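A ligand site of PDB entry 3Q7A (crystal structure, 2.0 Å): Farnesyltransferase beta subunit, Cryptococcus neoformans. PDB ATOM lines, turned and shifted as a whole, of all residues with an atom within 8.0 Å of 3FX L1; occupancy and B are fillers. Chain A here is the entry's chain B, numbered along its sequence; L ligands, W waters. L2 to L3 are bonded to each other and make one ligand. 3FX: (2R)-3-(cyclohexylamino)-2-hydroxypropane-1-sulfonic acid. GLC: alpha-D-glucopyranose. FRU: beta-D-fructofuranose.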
ATOM      1  N   TYR A  58       6.219 -16.149  19.991  1.00  0.00           N
ATOM      2  CA  TYR A  58       5.358 -15.250  19.226  1.00  0.00           C
ATOM      3  C   TYR A  58       5.214 -15.731  17.790  1.00  0.00           C
ATOM      4  O   TYR A  58       6.201 -16.074  17.134  1.00  0.00           O
ATOM      5  CB  TYR A  58       5.882 -13.807  19.293  1.00  0.00           C
ATOM      6  CG  TYR A  58       5.041 -12.820  18.523  1.00  0.00           C
ATOM      7  CD1 TYR A  58       5.589 -12.073  17.474  1.00  0.00           C
ATOM      8  CD2 TYR A  58       3.689 -12.631  18.823  1.00  0.00           C
ATOM      9  CE1 TYR A  58       4.812 -11.178  16.751  1.00  0.00           C
ATOM     10  CE2 TYR A  58       2.904 -11.737  18.106  1.00  0.00           C
ATOM     11  CZ  TYR A  58       3.468 -11.012  17.074  1.00  0.00           C
ATOM     12  OH  TYR A  58       2.703 -10.126  16.364  1.00  0.00           O
ATOM     13  N   GLY A  60       3.950 -14.134  15.066  1.00  0.00           N
ATOM     14  CA  GLY A  60       3.915 -13.110  14.012  1.00  0.00           C
ATOM     15  C   GLY A  60       4.690 -13.530  12.770  1.00  0.00           C
ATOM     16  O   GLY A  60       5.726 -14.189  12.871  1.00  0.00           O
ATOM     17  N   LEU A  61       4.174 -13.154  11.604  1.00  0.00           N
ATOM     18  CA  LEU A  61       4.847 -13.480  10.348  1.00  0.00           C
ATOM     19  C   LEU A  61       6.193 -12.770  10.289  1.00  0.00           C
ATOM     20  O   LEU A  61       6.272 -11.545  10.296  1.00  0.00           O
ATOM     21  CB  LEU A  61       3.972 -13.094   9.148  1.00  0.00           C
ATOM     22  CG  LEU A  61       4.506 -13.489   7.765  1.00  0.00           C
ATOM     23  CD1 LEU A  61       4.522 -15.007   7.575  1.00  0.00           C
ATOM     24  CD2 LEU A  61       3.667 -12.819   6.686  1.00  0.00           C
ATOM     25  N   ILE A 486      -7.283 -10.896   8.885  1.00  0.00           N
ATOM     26  CA  ILE A 486      -5.852 -11.028   9.127  1.00  0.00           C
ATOM     27  C   ILE A 486      -5.624 -11.493  10.561  1.00  0.00           C
ATOM     28  O   ILE A 486      -5.635 -10.684  11.502  1.00  0.00           O
ATOM     29  CB  ILE A 486      -5.071  -9.718   8.839  1.00  0.00           C
ATOM     30  CG1 ILE A 486      -5.542  -9.044   7.544  1.00  0.00           C
ATOM     31  CG2 ILE A 486      -3.562  -9.978   8.842  1.00  0.00           C
ATOM     32  CD1 ILE A 486      -5.256  -9.833   6.272  1.00  0.00           C
ATOM     33  N   VAL A 487      -5.411 -12.797  10.719  1.00  0.00           N
ATOM     34  CA  VAL A 487      -5.164 -13.402  12.034  1.00  0.00           C
ATOM     35  C   VAL A 487      -3.863 -12.868  12.638  1.00  0.00           C
ATOM     36  O   VAL A 487      -2.829 -12.872  11.982  1.00  0.00           O
ATOM     37  CB  VAL A 487      -5.145 -14.953  11.939  1.00  0.00           C
ATOM     38  CG1 VAL A 487      -4.688 -15.589  13.256  1.00  0.00           C
ATOM     39  CG2 VAL A 487      -6.522 -15.485  11.534  1.00  0.00           C
ATOM     40  N   GLY A 488      -3.944 -12.398  13.881  1.00  0.00           N
ATOM     41  CA  GLY A 488      -2.772 -11.899  14.591  1.00  0.00           C
ATOM     42  C   GLY A 488      -2.489 -10.423  14.403  1.00  0.00           C
ATOM     43  O   GLY A 488      -1.513  -9.900  14.931  1.00  0.00           O
ATOM     44  N   GLY A 489      -3.342  -9.748  13.635  1.00  0.00           N
ATOM     45  CA  GLY A 489      -3.211  -8.309  13.424  1.00  0.00           C
ATOM     46  C   GLY A 489      -2.636  -7.932  12.071  1.00  0.00           C
ATOM     47  O   GLY A 489      -2.046  -8.760  11.379  1.00  0.00           O
ATOM     48  N   LYS A 490      -2.795  -6.658  11.714  1.00  0.00           N
ATOM     49  CA  LYS A 490      -2.531  -6.182  10.357  1.00  0.00           C
ATOM     50  C   LYS A 490      -1.071  -6.276   9.903  1.00  0.00           C
ATOM     51  O   LYS A 490      -0.811  -6.298   8.703  1.00  0.00           O
ATOM     52  CB  LYS A 490      -3.090  -4.772  10.170  1.00  0.00           C
ATOM     53  CG  LYS A 490      -4.620  -4.742  10.142  1.00  0.00           C
ATOM     54  CD  LYS A 490      -5.176  -3.345  10.004  1.00  0.00           C
ATOM     55  CE  LYS A 490      -6.685  -3.383   9.825  1.00  0.00           C
ATOM     56  NZ  LYS A 490      -7.245  -2.017   9.611  1.00  0.00           N
ATOM     57  N   ASP A 491      -0.133  -6.377  10.847  1.00  0.00           N
ATOM     58  CA  ASP A 491       1.267  -6.592  10.488  1.00  0.00           C
ATOM     59  C   ASP A 491       1.525  -7.948   9.820  1.00  0.00           C
ATOM     60  O   ASP A 491       2.528  -8.134   9.134  1.00  0.00           O
ATOM     61  CB  ASP A 491       2.177  -6.398  11.703  1.00  0.00           C
ATOM     62  CG  ASP A 491       2.379  -4.937  12.065  1.00  0.00           C
ATOM     63  OD1 ASP A 491       2.464  -4.090  11.146  1.00  0.00           O
ATOM     64  OD2 ASP A 491       2.444  -4.633  13.265  1.00  0.00           O
ATOM     65  N   ASN A 492       0.607  -8.888  10.022  1.00  0.00           N
ATOM     66  CA  ASN A 492       0.661 -10.189   9.349  1.00  0.00           C
ATOM     67  C   ASN A 492       0.137 -10.201   7.912  1.00  0.00           C
ATOM     68  O   ASN A 492       0.264 -11.212   7.211  1.00  0.00           O
ATOM     69  CB  ASN A 492      -0.084 -11.247  10.163  1.00  0.00           C
ATOM     70  CG  ASN A 492       0.668 -11.654  11.414  1.00  0.00           C
ATOM     71  OD1 ASN A 492       1.872 -11.435  11.532  1.00  0.00           O
ATOM     72  ND2 ASN A 492      -0.047 -12.262  12.358  1.00  0.00           N
ATOM     73  N   ARG A 493      -0.444  -9.074   7.474  1.00  0.00           N
ATOM     74  CA  ARG A 493      -1.043  -8.975   6.144  1.00  0.00           C
ATOM     75  C   ARG A 493      -0.032  -9.125   5.016  1.00  0.00           C
ATOM     76  O   ARG A 493       0.985  -8.424   4.973  1.00  0.00           O
ATOM     77  CB  ARG A 493      -1.800  -7.641   5.965  1.00  0.00           C
ATOM     78  CG  ARG A 493      -2.585  -7.558   4.655  1.00  0.00           C
ATOM     79  CD  ARG A 493      -2.896  -6.130   4.248  1.00  0.00           C
ATOM     80  NE  ARG A 493      -3.663  -6.081   3.003  1.00  0.00           N
ATOM     81  CZ  ARG A 493      -3.134  -5.978   1.781  1.00  0.00           C
ATOM     82  NH1 ARG A 493      -1.819  -5.913   1.601  1.00  0.00           N
ATOM     83  NH2 ARG A 493      -3.923  -5.953   0.717  1.00  0.00           N
HETATM   84  OAA 3FX L   1      -4.666  -3.080  14.934  1.00  0.00           O
HETATM   85  OAB 3FX L   1      -3.954  -5.049  13.772  1.00  0.00           O
HETATM   86  OAC 3FX L   1      -0.786  -4.766  13.527  1.00  0.00           O
HETATM   87  OAD 3FX L   1      -3.110  -2.915  13.059  1.00  0.00           O
HETATM   88  CAE 3FX L   1       5.033  -5.699  17.382  1.00  0.00           C
HETATM   89  CAF 3FX L   1       3.991  -4.678  17.856  1.00  0.00           C
HETATM   90  CAG 3FX L   1       4.375  -7.036  16.999  1.00  0.00           C
HETATM   91  CAH 3FX L   1       2.916  -4.474  16.773  1.00  0.00           C
HETATM   92  CAI 3FX L   1       3.261  -6.838  15.946  1.00  0.00           C
HETATM   93  CAJ 3FX L   1      -0.017  -5.120  15.814  1.00  0.00           C
HETATM   94  CAK 3FX L   1      -2.162  -3.967  15.420  1.00  0.00           C
HETATM   95  NAL 3FX L   1       1.273  -5.569  15.282  1.00  0.00           N
HETATM   96  CAM 3FX L   1      -0.755  -4.199  14.852  1.00  0.00           C
HETATM   97  CAN 3FX L   1       2.218  -5.793  16.392  1.00  0.00           C
HETATM   98  SAO 3FX L   1      -3.526  -3.755  14.227  1.00  0.00           S
HETATM   99  C1  GLC L   2      -8.484  -8.946  14.813  1.00  0.00           C
HETATM  100  C2  GLC L   2      -7.738  -9.237  16.128  1.00  0.00           C
HETATM  101  C3  GLC L   2      -6.776 -10.414  15.978  1.00  0.00           C
HETATM  102  C4  GLC L   2      -7.479 -11.645  15.362  1.00  0.00           C
HETATM  103  C5  GLC L   2      -8.209 -11.247  14.072  1.00  0.00           C
HETATM  104  C6  GLC L   2      -8.959 -12.437  13.436  1.00  0.00           C
HETATM  105  O2  GLC L   2      -7.010  -8.070  16.534  1.00  0.00           O
HETATM  106  O3  GLC L   2      -6.222 -10.757  17.250  1.00  0.00           O
HETATM  107  O4  GLC L   2      -6.494 -12.650  15.096  1.00  0.00           O
HETATM  108  O5  GLC L   2      -9.127 -10.143  14.314  1.00  0.00           O
HETATM  109  O6  GLC L   2     -10.208 -12.641  14.103  1.00  0.00           O
HETATM  110  C1  FRU L   3      -7.552  -6.003  13.670  1.00  0.00           C
HETATM  111  C2  FRU L   3      -8.010  -7.315  13.024  1.00  0.00           C
HETATM  112  C3  FRU L   3      -7.449  -7.469  11.593  1.00  0.00           C
HETATM  113  C4  FRU L   3      -8.489  -8.389  10.984  1.00  0.00           C
HETATM  114  C5  FRU L   3      -9.759  -7.700  11.476  1.00  0.00           C
HETATM  115  C6  FRU L   3     -11.005  -8.610  11.393  1.00  0.00           C
HETATM  116  O1  FRU L   3      -8.076  -4.887  12.941  1.00  0.00           O
HETATM  117  O2  FRU L   3      -7.538  -8.415  13.838  1.00  0.00           O
HETATM  118  O3  FRU L   3      -6.160  -8.088  11.618  1.00  0.00           O
HETATM  119  O4  FRU L   3      -8.433  -8.368   9.562  1.00  0.00           O
HETATM  120  O5  FRU L   3      -9.459  -7.339  12.860  1.00  0.00           O
HETATM  121  O6  FRU L   3     -10.776  -9.805  12.153  1.00  0.00           O
HETATM  122  O   HOH W   1       5.128  -8.781  13.746  1.00  0.00           O
HETATM  123  O   HOH W   2      -7.174  -2.655  14.068  1.00  0.00           O
HETATM  124  O   HOH W   3       0.244  -8.019  13.980  1.00  0.00           O
HETATM  125  O   HOH W   4      -4.512  -6.762  16.159  1.00  0.00           O
HETATM  126  O   HOH W   5      -1.309  -7.551  17.025  1.00  0.00           O
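Merely in contact with 3FX L1: Tyr 58 (3.4 Å) and Gly 489 (3.4 Å).
Of the 11 residues printed, 4 come within 4 Å of 3FX L1.
The nearest printed residue that does not touch 3FX L1 is Gly 488 (5.1 Å).
Water W2 lies within hydrogen-bond range of an oxygen (O1) of FRU L3 (2.7 Å) and an oxygen (OAA) of 3FX L1 (2.7 Å).
Water W3 lies within hydrogen-bond range of the backbone carbonyl oxygen (O) of Gly 488 (2.7 Å) and a nitrogen (NAL) of 3FX L1 (3.0 Å).
Water W4 bridges O2 of GLC L2 and OAB of 3FX L1.
The backbone carbonyl oxygen of Ile 486 sits at hydrogen-bond distance from an oxygen (O3) of FRU L3 (2.7 Å).
The backbone NH (N) of Asp 491 lies within hydrogen-bond range of an oxygen (OAC) of 3FX L1, 3.2 Å away.
N of Gly 488 sits at hydrogen-bond distance from O4 of GLC L2, at 2.8 Å.
An oxygen (OAB) of 3FX L1 lies within hydrogen-bond range of the backbone NH (N) of Lys 490.
NAL of 3FX L1 lies within salt-bridge range of OD2 of Asp 491.
O4 of FRU L3 sits at hydrogen-bond distance from N of Ile 486, 2.9 Å away.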
